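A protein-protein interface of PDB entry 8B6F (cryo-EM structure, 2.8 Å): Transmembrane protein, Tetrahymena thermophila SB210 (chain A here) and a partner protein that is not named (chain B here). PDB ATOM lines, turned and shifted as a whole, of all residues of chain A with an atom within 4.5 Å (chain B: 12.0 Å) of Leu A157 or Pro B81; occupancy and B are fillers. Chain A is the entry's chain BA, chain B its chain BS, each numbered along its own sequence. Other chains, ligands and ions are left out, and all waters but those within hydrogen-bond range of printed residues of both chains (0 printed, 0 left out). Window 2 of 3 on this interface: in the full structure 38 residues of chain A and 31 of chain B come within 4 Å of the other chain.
NZ of Lys A118 is in hydrogen-bond range of O of Ser B78, at 2.7 Å.
The side-chain amide oxygen of Asn A161 lies close to the backbone carbonyl oxygen of Tyr B83, 3.0 Å away.
Pro B81 touches just these residues of chain A: Leu A110, Leu A157 and His A158.
Of chain B, only Ser B78 and Pro B80 come within 4 Å of Lys A118.
No residue of chain B comes within 4 Å of Ala A155.
Of chain B, only Tyr B83 (3.0 Å) comes within 4 Å of Asn A161.
Printed residues of chain A within 4 Å of Pro B80: Leu A110 and Lys A118.
Printed residues of chain B within 4 Å of Leu A110: Pro B80 (3.5 Å) and Pro B81 (3.3 Å).
Gln A153 touches none of the printed residues of chain B.
The nearest residue of chain B that does not touch Leu A157 is Pro B80 (5.3 Å).
The nearest residue of chain A that does not touch Pro B81 is Asn A161 (4.2 Å).
The backbone carbonyl oxygen (O) of Met A154 lies within hydrogen-bond range of a ring nitrogen (ND1) of His A158 (2.9 Å).
Printed residues of chain B that touch a printed residue of chain A: Ser B78, Pro B80, Pro B81 and Tyr B83.
Hydrophobic or aromatic side chains of chain A within 4 Å of the printed part of chain B: Leu A110 and His A158.
Among the printed residues, 8 pairs touch across the chains.
Leu A110 touches Pro B80.
CD1 of Leu A110 touches O of Pro B81 (3.3 Å).
Pro B80 touches Lys A118 (CD to NZ, 3.96 Å).
O of Leu A157 touches CG of Pro B81, 3.8 Å away.
His A158 touches Pro B81 (CD2 to CG, 3.9 Å).
His A158 touches Tyr B83 (CD2 to OH, 3.2 Å).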
ATOM      1  N   LEU A 110      -0.316  27.807  16.116  1.00  0.00           N
ATOM      2  CA  LEU A 110      -1.757  27.956  16.233  1.00  0.00           C
ATOM      3  C   LEU A 110      -2.175  29.379  15.871  1.00  0.00           C
ATOM      4  O   LEU A 110      -1.378  30.321  15.911  1.00  0.00           O
ATOM      5  CB  LEU A 110      -2.213  27.607  17.649  1.00  0.00           C
ATOM      6  CG  LEU A 110      -1.871  26.183  18.097  1.00  0.00           C
ATOM      7  CD1 LEU A 110      -2.170  25.998  19.572  1.00  0.00           C
ATOM      8  CD2 LEU A 110      -2.624  25.154  17.266  1.00  0.00           C
ATOM      9  N   LYS A 118     -10.818  28.221  21.925  1.00  0.00           N
ATOM     10  CA  LYS A 118     -10.472  27.841  23.291  1.00  0.00           C
ATOM     11  C   LYS A 118     -11.082  28.802  24.303  1.00  0.00           C
ATOM     12  O   LYS A 118     -11.655  28.377  25.311  1.00  0.00           O
ATOM     13  CB  LYS A 118      -8.950  27.791  23.436  1.00  0.00           C
ATOM     14  CG  LYS A 118      -8.447  27.429  24.829  1.00  0.00           C
ATOM     15  CD  LYS A 118      -8.236  28.665  25.694  1.00  0.00           C
ATOM     16  CE  LYS A 118      -7.441  28.340  26.948  1.00  0.00           C
ATOM     17  NZ  LYS A 118      -6.036  27.958  26.637  1.00  0.00           N
ATOM     18  N   PHE A 121     -14.831  28.493  24.569  1.00  0.00           N
ATOM     19  CA  PHE A 121     -15.125  27.347  25.423  1.00  0.00           C
ATOM     20  C   PHE A 121     -14.972  27.720  26.891  1.00  0.00           C
ATOM     21  O   PHE A 121     -15.816  27.375  27.724  1.00  0.00           O
ATOM     22  CB  PHE A 121     -14.209  26.176  25.064  1.00  0.00           C
ATOM     23  CG  PHE A 121     -14.490  25.563  23.717  1.00  0.00           C
ATOM     24  CD1 PHE A 121     -15.641  25.878  23.007  1.00  0.00           C
ATOM     25  CD2 PHE A 121     -13.601  24.655  23.169  1.00  0.00           C
ATOM     26  CE1 PHE A 121     -15.890  25.304  21.777  1.00  0.00           C
ATOM     27  CE2 PHE A 121     -13.845  24.079  21.939  1.00  0.00           C
ATOM     28  CZ  PHE A 121     -14.992  24.403  21.243  1.00  0.00           C
ATOM     29  N   GLN A 153     -14.901  19.712  24.609  1.00  0.00           N
ATOM     30  CA  GLN A 153     -14.065  20.865  24.294  1.00  0.00           C
ATOM     31  C   GLN A 153     -12.591  20.485  24.252  1.00  0.00           C
ATOM     32  O   GLN A 153     -11.864  20.888  23.337  1.00  0.00           O
ATOM     33  CB  GLN A 153     -14.298  21.970  25.320  1.00  0.00           C
ATOM     34  CG  GLN A 153     -15.687  22.587  25.260  1.00  0.00           C
ATOM     35  CD  GLN A 153     -16.003  23.471  26.458  1.00  0.00           C
ATOM     36  OE1 GLN A 153     -17.124  23.960  26.593  1.00  0.00           O
ATOM     37  NE2 GLN A 153     -15.021  23.683  27.332  1.00  0.00           N
ATOM     38  N   MET A 154     -12.129  19.703  25.228  1.00  0.00           N
ATOM     39  CA  MET A 154     -10.730  19.289  25.231  1.00  0.00           C
ATOM     40  C   MET A 154     -10.404  18.465  23.993  1.00  0.00           C
ATOM     41  O   MET A 154      -9.350  18.650  23.373  1.00  0.00           O
ATOM     42  CB  MET A 154     -10.418  18.497  26.500  1.00  0.00           C
ATOM     43  CG  MET A 154     -10.404  19.340  27.764  1.00  0.00           C
ATOM     44  SD  MET A 154      -9.739  18.458  29.192  1.00  0.00           S
ATOM     45  CE  MET A 154     -10.857  17.062  29.287  1.00  0.00           C
ATOM     46  N   ALA A 155     -11.296  17.547  23.619  1.00  0.00           N
ATOM     47  CA  ALA A 155     -11.070  16.747  22.422  1.00  0.00           C
ATOM     48  C   ALA A 155     -11.040  17.622  21.175  1.00  0.00           C
ATOM     49  O   ALA A 155     -10.202  17.421  20.287  1.00  0.00           O
ATOM     50  CB  ALA A 155     -12.152  15.675  22.299  1.00  0.00           C
ATOM     51  N   THR A 156     -11.946  18.598  21.090  1.00  0.00           N
ATOM     52  CA  THR A 156     -12.003  19.451  19.909  1.00  0.00           C
ATOM     53  C   THR A 156     -10.776  20.346  19.795  1.00  0.00           C
ATOM     54  O   THR A 156     -10.343  20.656  18.679  1.00  0.00           O
ATOM     55  CB  THR A 156     -13.270  20.306  19.941  1.00  0.00           C
ATOM     56  OG1 THR A 156     -14.425  19.457  19.927  1.00  0.00           O
ATOM     57  CG2 THR A 156     -13.326  21.244  18.737  1.00  0.00           C
ATOM     58  N   LEU A 157     -10.207  20.774  20.923  1.00  0.00           N
ATOM     59  CA  LEU A 157      -9.050  21.660  20.868  1.00  0.00           C
ATOM     60  C   LEU A 157      -7.886  21.024  20.119  1.00  0.00           C
ATOM     61  O   LEU A 157      -7.038  21.738  19.574  1.00  0.00           O
ATOM     62  CB  LEU A 157      -8.622  22.054  22.282  1.00  0.00           C
ATOM     63  CG  LEU A 157      -9.492  23.101  22.985  1.00  0.00           C
ATOM     64  CD1 LEU A 157      -9.016  23.318  24.410  1.00  0.00           C
ATOM     65  CD2 LEU A 157      -9.503  24.419  22.226  1.00  0.00           C
ATOM     66  N   HIS A 158      -7.820  19.693  20.086  1.00  0.00           N
ATOM     67  CA  HIS A 158      -6.773  19.020  19.329  1.00  0.00           C
ATOM     68  C   HIS A 158      -7.044  19.011  17.831  1.00  0.00           C
ATOM     69  O   HIS A 158      -6.104  18.845  17.048  1.00  0.00           O
ATOM     70  CB  HIS A 158      -6.610  17.577  19.814  1.00  0.00           C
ATOM     71  CG  HIS A 158      -6.082  17.463  21.210  1.00  0.00           C
ATOM     72  ND1 HIS A 158      -6.858  17.712  22.322  1.00  0.00           N
ATOM     73  CD2 HIS A 158      -4.857  17.123  21.674  1.00  0.00           C
ATOM     74  CE1 HIS A 158      -6.132  17.532  23.411  1.00  0.00           C
ATOM     75  NE2 HIS A 158      -4.914  17.174  23.046  1.00  0.00           N
ATOM     76  N   ILE A 159      -8.300  19.185  17.413  1.00  0.00           N
ATOM     77  CA  ILE A 159      -8.637  19.022  15.999  1.00  0.00           C
ATOM     78  C   ILE A 159      -7.874  20.004  15.118  1.00  0.00           C
ATOM     79  O   ILE A 159      -7.345  19.583  14.076  1.00  0.00           O
ATOM     80  CB  ILE A 159     -10.161  19.112  15.807  1.00  0.00           C
ATOM     81  CG1 ILE A 159     -10.834  17.884  16.427  1.00  0.00           C
ATOM     82  CG2 ILE A 159     -10.516  19.231  14.324  1.00  0.00           C
ATOM     83  CD1 ILE A 159     -12.350  17.946  16.443  1.00  0.00           C
ATOM     84  N   PRO A 160      -7.776  21.294  15.451  1.00  0.00           N
ATOM     85  CA  PRO A 160      -7.019  22.201  14.570  1.00  0.00           C
ATOM     86  C   PRO A 160      -5.586  21.759  14.347  1.00  0.00           C
ATOM     87  O   PRO A 160      -5.083  21.854  13.222  1.00  0.00           O
ATOM     88  CB  PRO A 160      -7.095  23.545  15.308  1.00  0.00           C
ATOM     89  CG  PRO A 160      -8.319  23.454  16.139  1.00  0.00           C
ATOM     90  CD  PRO A 160      -8.431  22.018  16.553  1.00  0.00           C
ATOM     91  N   ASN A 161      -4.906  21.282  15.391  1.00  0.00           N
ATOM     92  CA  ASN A 161      -3.524  20.847  15.228  1.00  0.00           C
ATOM     93  C   ASN A 161      -3.432  19.630  14.318  1.00  0.00           C
ATOM     94  O   ASN A 161      -2.560  19.565  13.445  1.00  0.00           O
ATOM     95  CB  ASN A 161      -2.906  20.541  16.591  1.00  0.00           C
ATOM     96  CG  ASN A 161      -1.481  20.050  16.481  1.00  0.00           C
ATOM     97  OD1 ASN A 161      -0.789  20.331  15.505  1.00  0.00           O
ATOM     98  ND2 ASN A 161      -1.032  19.309  17.485  1.00  0.00           N
ATOM     99  N   TYR B  64      -3.383  40.386  21.158  1.00  0.00           N
ATOM    100  CA  TYR B  64      -2.944  39.149  20.523  1.00  0.00           C
ATOM    101  C   TYR B  64      -1.422  39.051  20.473  1.00  0.00           C
ATOM    102  O   TYR B  64      -0.834  38.106  21.008  1.00  0.00           O
ATOM    103  CB  TYR B  64      -3.544  39.055  19.119  1.00  0.00           C
ATOM    104  CG  TYR B  64      -3.372  37.710  18.453  1.00  0.00           C
ATOM    105  CD1 TYR B  64      -4.015  36.584  18.948  1.00  0.00           C
ATOM    106  CD2 TYR B  64      -2.591  37.573  17.315  1.00  0.00           C
ATOM    107  CE1 TYR B  64      -3.870  35.354  18.336  1.00  0.00           C
ATOM    108  CE2 TYR B  64      -2.441  36.349  16.696  1.00  0.00           C
ATOM    109  CZ  TYR B  64      -3.082  35.244  17.211  1.00  0.00           C
ATOM    110  OH  TYR B  64      -2.932  34.025  16.594  1.00  0.00           O
ATOM    111  N   MET B  77      -1.509  31.269  31.300  1.00  0.00           N
ATOM    112  CA  MET B  77      -2.634  30.353  31.219  1.00  0.00           C
ATOM    113  C   MET B  77      -2.259  29.121  30.402  1.00  0.00           C
ATOM    114  O   MET B  77      -1.256  29.099  29.687  1.00  0.00           O
ATOM    115  CB  MET B  77      -3.844  31.051  30.597  1.00  0.00           C
ATOM    116  CG  MET B  77      -4.200  32.366  31.278  1.00  0.00           C
ATOM    117  SD  MET B  77      -4.462  32.165  33.049  1.00  0.00           S
ATOM    118  CE  MET B  77      -4.339  33.857  33.616  1.00  0.00           C
ATOM    119  N   SER B  78      -3.084  28.083  30.524  1.00  0.00           N
ATOM    120  CA  SER B  78      -2.823  26.837  29.816  1.00  0.00           C
ATOM    121  C   SER B  78      -2.759  27.088  28.316  1.00  0.00           C
ATOM    122  O   SER B  78      -3.618  27.767  27.750  1.00  0.00           O
ATOM    123  CB  SER B  78      -3.907  25.807  30.135  1.00  0.00           C
ATOM    124  OG  SER B  78      -5.185  26.278  29.747  1.00  0.00           O
ATOM    125  N   GLN B  79      -1.734  26.533  27.676  1.00  0.00           N
ATOM    126  CA  GLN B  79      -1.553  26.756  26.249  1.00  0.00           C
ATOM    127  C   GLN B  79      -2.271  25.670  25.448  1.00  0.00           C
ATOM    128  O   GLN B  79      -2.190  24.488  25.799  1.00  0.00           O
ATOM    129  CB  GLN B  79      -0.070  26.753  25.894  1.00  0.00           C
ATOM    130  CG  GLN B  79       0.276  27.514  24.622  1.00  0.00           C
ATOM    131  CD  GLN B  79      -0.015  29.003  24.719  1.00  0.00           C
ATOM    132  OE1 GLN B  79      -0.459  29.620  23.752  1.00  0.00           O
ATOM    133  NE2 GLN B  79       0.244  29.591  25.884  1.00  0.00           N
ATOM    134  N   PRO B  80      -2.979  26.020  24.377  1.00  0.00           N
ATOM    135  CA  PRO B  80      -3.642  24.990  23.582  1.00  0.00           C
ATOM    136  C   PRO B  80      -2.623  24.047  22.974  1.00  0.00           C
ATOM    137  O   PRO B  80      -1.472  24.437  22.704  1.00  0.00           O
ATOM    138  CB  PRO B  80      -4.389  25.795  22.508  1.00  0.00           C
ATOM    139  CG  PRO B  80      -3.745  27.129  22.488  1.00  0.00           C
ATOM    140  CD  PRO B  80      -3.264  27.375  23.874  1.00  0.00           C
ATOM    141  N   PRO B  81      -3.000  22.789  22.743  1.00  0.00           N
ATOM    142  CA  PRO B  81      -2.014  21.793  22.305  1.00  0.00           C
ATOM    143  C   PRO B  81      -1.348  22.183  20.994  1.00  0.00           C
ATOM    144  O   PRO B  81      -1.986  22.711  20.082  1.00  0.00           O
ATOM    145  CB  PRO B  81      -2.845  20.513  22.158  1.00  0.00           C
ATOM    146  CG  PRO B  81      -4.243  20.984  21.959  1.00  0.00           C
ATOM    147  CD  PRO B  81      -4.367  22.241  22.764  1.00  0.00           C
ATOM    148  N   LYS B  82      -0.050  21.902  20.906  1.00  0.00           N
ATOM    149  CA  LYS B  82       0.732  22.212  19.712  1.00  0.00           C
ATOM    150  C   LYS B  82       1.857  21.191  19.615  1.00  0.00           C
ATOM    151  O   LYS B  82       2.780  21.208  20.434  1.00  0.00           O
ATOM    152  CB  LYS B  82       1.284  23.634  19.770  1.00  0.00           C
ATOM    153  CG  LYS B  82       2.201  23.995  18.610  1.00  0.00           C
ATOM    154  CD  LYS B  82       2.694  25.428  18.723  1.00  0.00           C
ATOM    155  CE  LYS B  82       3.709  25.747  17.639  1.00  0.00           C
ATOM    156  NZ  LYS B  82       4.161  27.165  17.698  1.00  0.00           N
ATOM    157  N   TYR B  83       1.780  20.309  18.622  1.00  0.00           N
ATOM    158  CA  TYR B  83       2.771  19.256  18.454  1.00  0.00           C
ATOM    159  C   TYR B  83       2.717  18.763  17.017  1.00  0.00           C
ATOM    160  O   TYR B  83       1.753  19.018  16.291  1.00  0.00           O
ATOM    161  CB  TYR B  83       2.531  18.102  19.433  1.00  0.00           C
ATOM    162  CG  TYR B  83       1.110  17.592  19.421  1.00  0.00           C
ATOM    163  CD1 TYR B  83       0.150  18.138  20.262  1.00  0.00           C
ATOM    164  CD2 TYR B  83       0.726  16.573  18.561  1.00  0.00           C
ATOM    165  CE1 TYR B  83      -1.153  17.677  20.251  1.00  0.00           C
ATOM    166  CE2 TYR B  83      -0.572  16.107  18.542  1.00  0.00           C
ATOM    167  CZ  TYR B  83      -1.507  16.663  19.388  1.00  0.00           C
ATOM    168  OH  TYR B  83      -2.802  16.200  19.371  1.00  0.00           O
ATOM    169  N   ASP B  84       3.767  18.055  16.615  1.00  0.00           N
ATOM    170  CA  ASP B  84       3.860  17.467  15.288  1.00  0.00           C
ATOM    171  C   ASP B  84       3.787  15.950  15.389  1.00  0.00           C
ATOM    172  O   ASP B  84       4.259  15.351  16.360  1.00  0.00           O
ATOM    173  CB  ASP B  84       5.156  17.880  14.582  1.00  0.00           C
ATOM    174  CG  ASP B  84       6.394  17.394  15.302  1.00  0.00           C
ATOM    175  OD1 ASP B  84       6.659  16.175  15.273  1.00  0.00           O
ATOM    176  OD2 ASP B  84       7.106  18.230  15.895  1.00  0.00           O
ATOM    177  N   LEU B  85       3.190  15.332  14.369  1.00  0.00           N
ATOM    178  CA  LEU B  85       2.989  13.889  14.325  1.00  0.00           C
ATOM    179  C   LEU B  85       4.092  13.176  13.552  1.00  0.00           C
ATOM    180  O   LEU B  85       3.852  12.119  12.959  1.00  0.00           O
ATOM    181  CB  LEU B  85       1.626  13.569  13.716  1.00  0.00           C
ATOM    182  CG  LEU B  85       0.421  14.230  14.390  1.00  0.00           C
ATOM    183  CD1 LEU B  85      -0.858  13.884  13.647  1.00  0.00           C
ATOM    184  CD2 LEU B  85       0.321  13.820  15.852  1.00  0.00           C
